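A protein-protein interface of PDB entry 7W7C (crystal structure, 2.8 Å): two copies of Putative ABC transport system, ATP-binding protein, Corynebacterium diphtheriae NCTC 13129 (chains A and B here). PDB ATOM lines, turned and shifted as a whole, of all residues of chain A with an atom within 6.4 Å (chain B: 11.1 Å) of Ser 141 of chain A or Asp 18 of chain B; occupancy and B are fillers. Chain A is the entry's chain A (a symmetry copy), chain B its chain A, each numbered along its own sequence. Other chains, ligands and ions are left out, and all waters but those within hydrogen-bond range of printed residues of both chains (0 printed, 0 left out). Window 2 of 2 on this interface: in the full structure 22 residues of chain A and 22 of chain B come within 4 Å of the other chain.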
ATOM      1  N   VAL A 137     -15.307 -22.975   9.761  1.00  0.00           N
ATOM      2  CA  VAL A 137     -13.995 -23.577   9.995  1.00  0.00           C
ATOM      3  C   VAL A 137     -13.550 -24.396   8.788  1.00  0.00           C
ATOM      4  O   VAL A 137     -12.362 -24.416   8.439  1.00  0.00           O
ATOM      5  CB  VAL A 137     -14.022 -24.419  11.285  1.00  0.00           C
ATOM      6  CG1 VAL A 137     -12.763 -25.257  11.409  1.00  0.00           C
ATOM      7  CG2 VAL A 137     -14.181 -23.520  12.499  1.00  0.00           C
ATOM      8  N   ALA A 138     -14.494 -25.059   8.115  1.00  0.00           N
ATOM      9  CA  ALA A 138     -14.147 -25.842   6.935  1.00  0.00           C
ATOM     10  C   ALA A 138     -13.591 -24.980   5.810  1.00  0.00           C
ATOM     11  O   ALA A 138     -12.918 -25.508   4.913  1.00  0.00           O
ATOM     12  CB  ALA A 138     -15.371 -26.616   6.437  1.00  0.00           C
ATOM     13  N   GLN A 139     -13.846 -23.672   5.838  1.00  0.00           N
ATOM     14  CA  GLN A 139     -13.378 -22.771   4.795  1.00  0.00           C
ATOM     15  C   GLN A 139     -12.034 -22.127   5.108  1.00  0.00           C
ATOM     16  O   GLN A 139     -11.501 -21.412   4.256  1.00  0.00           O
ATOM     17  CB  GLN A 139     -14.424 -21.682   4.530  1.00  0.00           C
ATOM     18  CG  GLN A 139     -15.622 -22.169   3.723  1.00  0.00           C
ATOM     19  CD  GLN A 139     -16.930 -22.106   4.501  1.00  0.00           C
ATOM     20  OE1 GLN A 139     -17.251 -21.094   5.127  1.00  0.00           O
ATOM     21  NE2 GLN A 139     -17.688 -23.199   4.473  1.00  0.00           N
ATOM     22  N   LEU A 140     -11.461 -22.377   6.284  1.00  0.00           N
ATOM     23  CA  LEU A 140     -10.197 -21.771   6.683  1.00  0.00           C
ATOM     24  C   LEU A 140      -9.053 -22.758   6.493  1.00  0.00           C
ATOM     25  O   LEU A 140      -9.159 -23.923   6.885  1.00  0.00           O
ATOM     26  CB  LEU A 140     -10.245 -21.313   8.143  1.00  0.00           C
ATOM     27  CG  LEU A 140     -11.227 -20.202   8.518  1.00  0.00           C
ATOM     28  CD1 LEU A 140     -11.091 -19.875  10.000  1.00  0.00           C
ATOM     29  CD2 LEU A 140     -10.992 -18.969   7.668  1.00  0.00           C
ATOM     30  N   SER A 141      -7.969 -22.285   5.887  1.00  0.00           N
ATOM     31  CA  SER A 141      -6.767 -23.091   5.759  1.00  0.00           C
ATOM     32  C   SER A 141      -6.042 -23.173   7.104  1.00  0.00           C
ATOM     33  O   SER A 141      -6.254 -22.355   8.005  1.00  0.00           O
ATOM     34  CB  SER A 141      -5.841 -22.497   4.699  1.00  0.00           C
ATOM     35  OG  SER A 141      -5.289 -21.263   5.125  1.00  0.00           O
ATOM     36  N   GLY A 142      -5.161 -24.172   7.229  1.00  0.00           N
ATOM     37  CA  GLY A 142      -4.467 -24.380   8.497  1.00  0.00           C
ATOM     38  C   GLY A 142      -3.771 -23.131   9.003  1.00  0.00           C
ATOM     39  O   GLY A 142      -3.792 -22.835  10.204  1.00  0.00           O
ATOM     40  N   GLY A 143      -3.159 -22.371   8.092  1.00  0.00           N
ATOM     41  CA  GLY A 143      -2.593 -21.092   8.482  1.00  0.00           C
ATOM     42  C   GLY A 143      -3.636 -20.142   9.033  1.00  0.00           C
ATOM     43  O   GLY A 143      -3.452 -19.540  10.099  1.00  0.00           O
ATOM     44  N   GLN A 144      -4.762 -20.011   8.319  1.00  0.00           N
ATOM     45  CA  GLN A 144      -5.828 -19.117   8.767  1.00  0.00           C
ATOM     46  C   GLN A 144      -6.442 -19.594  10.073  1.00  0.00           C
ATOM     47  O   GLN A 144      -6.801 -18.780  10.936  1.00  0.00           O
ATOM     48  CB  GLN A 144      -6.901 -19.004   7.690  1.00  0.00           C
ATOM     49  CG  GLN A 144      -6.338 -18.563   6.359  1.00  0.00           C
ATOM     50  CD  GLN A 144      -7.412 -18.301   5.323  1.00  0.00           C
ATOM     51  OE1 GLN A 144      -8.304 -19.126   5.122  1.00  0.00           O
ATOM     52  NE2 GLN A 144      -7.333 -17.140   4.657  1.00  0.00           N
ATOM     53  N   ARG A 145      -6.595 -20.911  10.225  1.00  0.00           N
ATOM     54  CA  ARG A 145      -7.052 -21.477  11.489  1.00  0.00           C
ATOM     55  C   ARG A 145      -6.151 -21.044  12.635  1.00  0.00           C
ATOM     56  O   ARG A 145      -6.627 -20.623  13.695  1.00  0.00           O
ATOM     57  CB  ARG A 145      -7.079 -22.999  11.401  1.00  0.00           C
ATOM     58  CG  ARG A 145      -7.988 -23.533  10.332  1.00  0.00           C
ATOM     59  CD  ARG A 145      -9.198 -24.208  10.925  1.00  0.00           C
ATOM     60  NE  ARG A 145      -9.826 -25.068   9.934  1.00  0.00           N
ATOM     61  CZ  ARG A 145      -9.383 -26.279   9.618  1.00  0.00           C
ATOM     62  NH1 ARG A 145      -8.303 -26.770  10.221  1.00  0.00           N
ATOM     63  NH2 ARG A 145     -10.020 -26.988   8.694  1.00  0.00           N
ATOM     64  N   GLN A 146      -4.837 -21.168  12.446  1.00  0.00           N
ATOM     65  CA  GLN A 146      -3.912 -20.766  13.498  1.00  0.00           C
ATOM     66  C   GLN A 146      -4.016 -19.271  13.791  1.00  0.00           C
ATOM     67  O   GLN A 146      -3.936 -18.848  14.953  1.00  0.00           O
ATOM     68  CB  GLN A 146      -2.482 -21.150  13.113  1.00  0.00           C
ATOM     69  CG  GLN A 146      -2.066 -22.545  13.559  1.00  0.00           C
ATOM     70  CD  GLN A 146      -1.986 -22.669  15.070  1.00  0.00           C
ATOM     71  OE1 GLN A 146      -2.141 -21.688  15.798  1.00  0.00           O
ATOM     72  NE2 GLN A 146      -1.735 -23.885  15.551  1.00  0.00           N
ATOM     73  N   LEU A 170       2.713 -26.482   9.547  1.00  0.00           N
ATOM     74  CA  LEU A 170       2.789 -25.433   8.542  1.00  0.00           C
ATOM     75  C   LEU A 170       4.152 -25.441   7.852  1.00  0.00           C
ATOM     76  O   LEU A 170       5.149 -25.898   8.419  1.00  0.00           O
ATOM     77  CB  LEU A 170       2.547 -24.060   9.162  1.00  0.00           C
ATOM     78  CG  LEU A 170       1.223 -23.821   9.890  1.00  0.00           C
ATOM     79  CD1 LEU A 170       1.126 -22.360  10.302  1.00  0.00           C
ATOM     80  CD2 LEU A 170       0.061 -24.202   9.017  1.00  0.00           C
ATOM     81  N   LEU A 174       4.594 -20.021   5.973  1.00  0.00           N
ATOM     82  CA  LEU A 174       3.549 -19.803   6.966  1.00  0.00           C
ATOM     83  C   LEU A 174       4.111 -19.829   8.380  1.00  0.00           C
ATOM     84  O   LEU A 174       3.662 -19.065   9.239  1.00  0.00           O
ATOM     85  CB  LEU A 174       2.449 -20.850   6.819  1.00  0.00           C
ATOM     86  CG  LEU A 174       1.726 -20.857   5.480  1.00  0.00           C
ATOM     87  CD1 LEU A 174       0.561 -21.834   5.537  1.00  0.00           C
ATOM     88  CD2 LEU A 174       1.263 -19.463   5.105  1.00  0.00           C
ATOM     89  N   VAL B  14       1.409 -35.811  -2.252  1.00  0.00           N
ATOM     90  CA  VAL B  14       0.147 -35.800  -1.528  1.00  0.00           C
ATOM     91  C   VAL B  14      -0.357 -34.364  -1.531  1.00  0.00           C
ATOM     92  O   VAL B  14       0.291 -33.479  -0.951  1.00  0.00           O
ATOM     93  CB  VAL B  14       0.290 -36.340  -0.098  1.00  0.00           C
ATOM     94  CG1 VAL B  14      -1.018 -36.175   0.662  1.00  0.00           C
ATOM     95  CG2 VAL B  14       0.687 -37.802  -0.132  1.00  0.00           C
ATOM     96  N   VAL B  15      -1.481 -34.133  -2.217  1.00  0.00           N
ATOM     97  CA  VAL B  15      -2.186 -32.853  -2.248  1.00  0.00           C
ATOM     98  C   VAL B  15      -3.499 -33.026  -1.490  1.00  0.00           C
ATOM     99  O   VAL B  15      -4.301 -33.910  -1.815  1.00  0.00           O
ATOM    100  CB  VAL B  15      -2.443 -32.374  -3.687  1.00  0.00           C
ATOM    101  CG1 VAL B  15      -3.260 -31.085  -3.687  1.00  0.00           C
ATOM    102  CG2 VAL B  15      -1.128 -32.182  -4.430  1.00  0.00           C
ATOM    103  N   TYR B  16      -3.705 -32.187  -0.462  1.00  0.00           N
ATOM    104  CA  TYR B  16      -4.853 -32.122   0.430  1.00  0.00           C
ATOM    105  C   TYR B  16      -5.680 -30.875   0.147  1.00  0.00           C
ATOM    106  O   TYR B  16      -5.129 -29.831  -0.212  1.00  0.00           O
ATOM    107  CB  TYR B  16      -4.429 -32.052   1.901  1.00  0.00           C
ATOM    108  CG  TYR B  16      -3.837 -33.294   2.522  1.00  0.00           C
ATOM    109  CD1 TYR B  16      -4.384 -34.551   2.291  1.00  0.00           C
ATOM    110  CD2 TYR B  16      -2.750 -33.195   3.382  1.00  0.00           C
ATOM    111  CE1 TYR B  16      -3.846 -35.678   2.890  1.00  0.00           C
ATOM    112  CE2 TYR B  16      -2.210 -34.306   3.981  1.00  0.00           C
ATOM    113  CZ  TYR B  16      -2.757 -35.546   3.734  1.00  0.00           C
ATOM    114  OH  TYR B  16      -2.203 -36.645   4.344  1.00  0.00           O
ATOM    115  N   PRO B  17      -6.998 -30.932   0.338  1.00  0.00           N
ATOM    116  CA  PRO B  17      -7.776 -29.688   0.413  1.00  0.00           C
ATOM    117  C   PRO B  17      -7.499 -28.984   1.735  1.00  0.00           C
ATOM    118  O   PRO B  17      -7.664 -29.567   2.808  1.00  0.00           O
ATOM    119  CB  PRO B  17      -9.228 -30.171   0.313  1.00  0.00           C
ATOM    120  CG  PRO B  17      -9.195 -31.553   0.873  1.00  0.00           C
ATOM    121  CD  PRO B  17      -7.847 -32.128   0.491  1.00  0.00           C
ATOM    122  N   ASP B  18      -7.065 -27.729   1.659  1.00  0.00           N
ATOM    123  CA  ASP B  18      -6.779 -26.918   2.843  1.00  0.00           C
ATOM    124  C   ASP B  18      -7.789 -25.777   2.886  1.00  0.00           C
ATOM    125  O   ASP B  18      -7.527 -24.689   2.365  1.00  0.00           O
ATOM    126  CB  ASP B  18      -5.346 -26.391   2.814  1.00  0.00           C
ATOM    127  CG  ASP B  18      -4.867 -25.922   4.172  1.00  0.00           C
ATOM    128  OD1 ASP B  18      -5.469 -26.329   5.193  1.00  0.00           O
ATOM    129  OD2 ASP B  18      -3.889 -25.143   4.214  1.00  0.00           O
ATOM    130  N   GLY B  19      -8.937 -26.019   3.513  1.00  0.00           N
ATOM    131  CA  GLY B  19     -10.009 -25.035   3.474  1.00  0.00           C
ATOM    132  C   GLY B  19     -10.573 -24.938   2.071  1.00  0.00           C
ATOM    133  O   GLY B  19     -10.937 -25.947   1.456  1.00  0.00           O
ATOM    134  N   ILE B  20     -10.650 -23.712   1.544  1.00  0.00           N
ATOM    135  CA  ILE B  20     -11.055 -23.521   0.153  1.00  0.00           C
ATOM    136  C   ILE B  20      -9.899 -23.700  -0.819  1.00  0.00           C
ATOM    137  O   ILE B  20     -10.135 -23.878  -2.024  1.00  0.00           O
ATOM    138  CB  ILE B  20     -11.663 -22.129  -0.074  1.00  0.00           C
ATOM    139  CG1 ILE B  20     -10.665 -21.061   0.375  1.00  0.00           C
ATOM    140  CG2 ILE B  20     -12.999 -22.003   0.634  1.00  0.00           C
ATOM    141  CD1 ILE B  20     -11.262 -19.719   0.588  1.00  0.00           C
ATOM    142  N   SER B  21      -8.663 -23.640  -0.345  1.00  0.00           N
ATOM    143  CA  SER B  21      -7.514 -23.823  -1.212  1.00  0.00           C
ATOM    144  C   SER B  21      -7.008 -25.261  -1.087  1.00  0.00           C
ATOM    145  O   SER B  21      -7.740 -26.156  -0.650  1.00  0.00           O
ATOM    146  CB  SER B  21      -6.440 -22.788  -0.866  1.00  0.00           C
ATOM    147  OG  SER B  21      -6.218 -22.739   0.532  1.00  0.00           O
ATOM    148  N   THR B  22      -5.758 -25.489  -1.487  1.00  0.00           N
ATOM    149  CA  THR B  22      -5.118 -26.791  -1.383  1.00  0.00           C
ATOM    150  C   THR B  22      -3.732 -26.612  -0.788  1.00  0.00           C
ATOM    151  O   THR B  22      -3.132 -25.538  -0.867  1.00  0.00           O
ATOM    152  CB  THR B  22      -5.008 -27.492  -2.746  1.00  0.00           C
ATOM    153  OG1 THR B  22      -4.150 -26.735  -3.610  1.00  0.00           O
ATOM    154  CG2 THR B  22      -6.374 -27.624  -3.384  1.00  0.00           C
ATOM    155  N   VAL B  23      -3.225 -27.685  -0.189  1.00  0.00           N
ATOM    156  CA  VAL B  23      -1.872 -27.720   0.347  1.00  0.00           C
ATOM    157  C   VAL B  23      -1.181 -28.956  -0.195  1.00  0.00           C
ATOM    158  O   VAL B  23      -1.767 -30.042  -0.222  1.00  0.00           O
ATOM    159  CB  VAL B  23      -1.873 -27.704   1.894  1.00  0.00           C
ATOM    160  CG1 VAL B  23      -2.815 -28.778   2.436  1.00  0.00           C
ATOM    161  CG2 VAL B  23      -0.463 -27.894   2.444  1.00  0.00           C
ATOM    162  N   THR B  24       0.060 -28.789  -0.645  1.00  0.00           N
ATOM    163  CA  THR B  24       0.842 -29.896  -1.187  1.00  0.00           C
ATOM    164  C   THR B  24       1.659 -30.472  -0.040  1.00  0.00           C
ATOM    165  O   THR B  24       2.798 -30.075   0.209  1.00  0.00           O
ATOM    166  CB  THR B  24       1.709 -29.436  -2.352  1.00  0.00           C
ATOM    167  OG1 THR B  24       0.868 -28.943  -3.398  1.00  0.00           O
ATOM    168  CG2 THR B  24       2.526 -30.593  -2.885  1.00  0.00           C
ATOM    169  N   ALA B  25       1.041 -31.419   0.677  1.00  0.00           N
ATOM    170  CA  ALA B  25       1.675 -32.020   1.845  1.00  0.00           C
ATOM    171  C   ALA B  25       2.956 -32.750   1.478  1.00  0.00           C
ATOM    172  O   ALA B  25       3.867 -32.854   2.308  1.00  0.00           O
ATOM    173  CB  ALA B  25       0.699 -32.974   2.535  1.00  0.00           C
ATOM    174  N   GLY B  46       6.264 -29.761  10.107  1.00  0.00           N
ATOM    175  CA  GLY B  46       5.479 -29.260   8.996  1.00  0.00           C
ATOM    176  C   GLY B  46       6.144 -29.338   7.639  1.00  0.00           C
ATOM    177  O   GLY B  46       5.723 -28.629   6.720  1.00  0.00           O
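No position is printed for both chains.
The side-chain hydroxyl (OG) of Ser 21 of chain B lies within hydrogen-bond range of the backbone carbonyl oxygen (O) of Asp 18 of chain B. NE of Arg 145 of chain A lies within hydrogen-bond range of O of Leu 140 of chain A (3.3 Å). The side-chain amide oxygen (OE1) of Gln 144 of chain A is in hydrogen-bond range of the backbone NH (N) of Ser 141 of chain A, 3.3 Å away.
Val 137 of chain A touches none of the printed residues of chain B. Printed residues of chain B within 4 Å of Gln 139 of chain A: Gly 19 (3.9 Å) and Ile 20 (3.7 Å). Leu 140 of chain A touches just one residue of chain B: Gly 19 (3.7 Å). Ser 141 of chain A touches one residue of chain B. Gly 142 of chain A touches just one residue of chain B: Asp 18. No residue of chain B comes within 4 Å of Gly 143 of chain A. Arg 145 of chain A touches none of the printed residues of chain B. Printed residues of chain B within 4 Å of Leu 170 of chain A: Gly 46. Printed residues of chain A within 4 Å of Gly 19 of chain B: Ala 138, Gln 139 and Leu 140. Printed residues of chain A within 4 Å of Ile 20 of chain B: Gln 139. Printed residues of chain A within 4 Å of Gly 46 of chain B: Leu 170. The nearest printed residue of chain B that does not touch Ser 141 of chain A is Gly 19 of chain B (4.2 Å).
Of the 13 printed residues of chain B, 4 touch a printed residue of chain A. Along chain B the printed residues that touch a printed residue of chain A span positions 18 to 46. Among the printed residues, no Asp or Glu carboxylate lies within 4 Å of a Lys or Arg side-chain nitrogen of the other chain.
Among the printed residues, merely in contact across the chains: Ala 138 of chain A with Gly 19 of chain B (3.3 Å), Ser 141 of chain A with Asp 18 of chain B (3.3 Å), Gln 139 of chain A with Ile 20 of chain B (3.7 Å), Leu 140 of chain A with Gly 19 of chain B (3.7 Å) and Gln 139 of chain A with Gly 19 of chain B (3.9 Å).
The backbone NH (N) of Gly 142 of chain A sits at hydrogen-bond distance from the side-chain carboxylate (OD1) of Asp 18 of chain B, at 3.0 Å. The backbone carbonyl oxygen (O) of Gly 46 of chain B sits close to the backbone carbonyl oxygen (O) of Leu 170 of chain A (3.3 Å).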
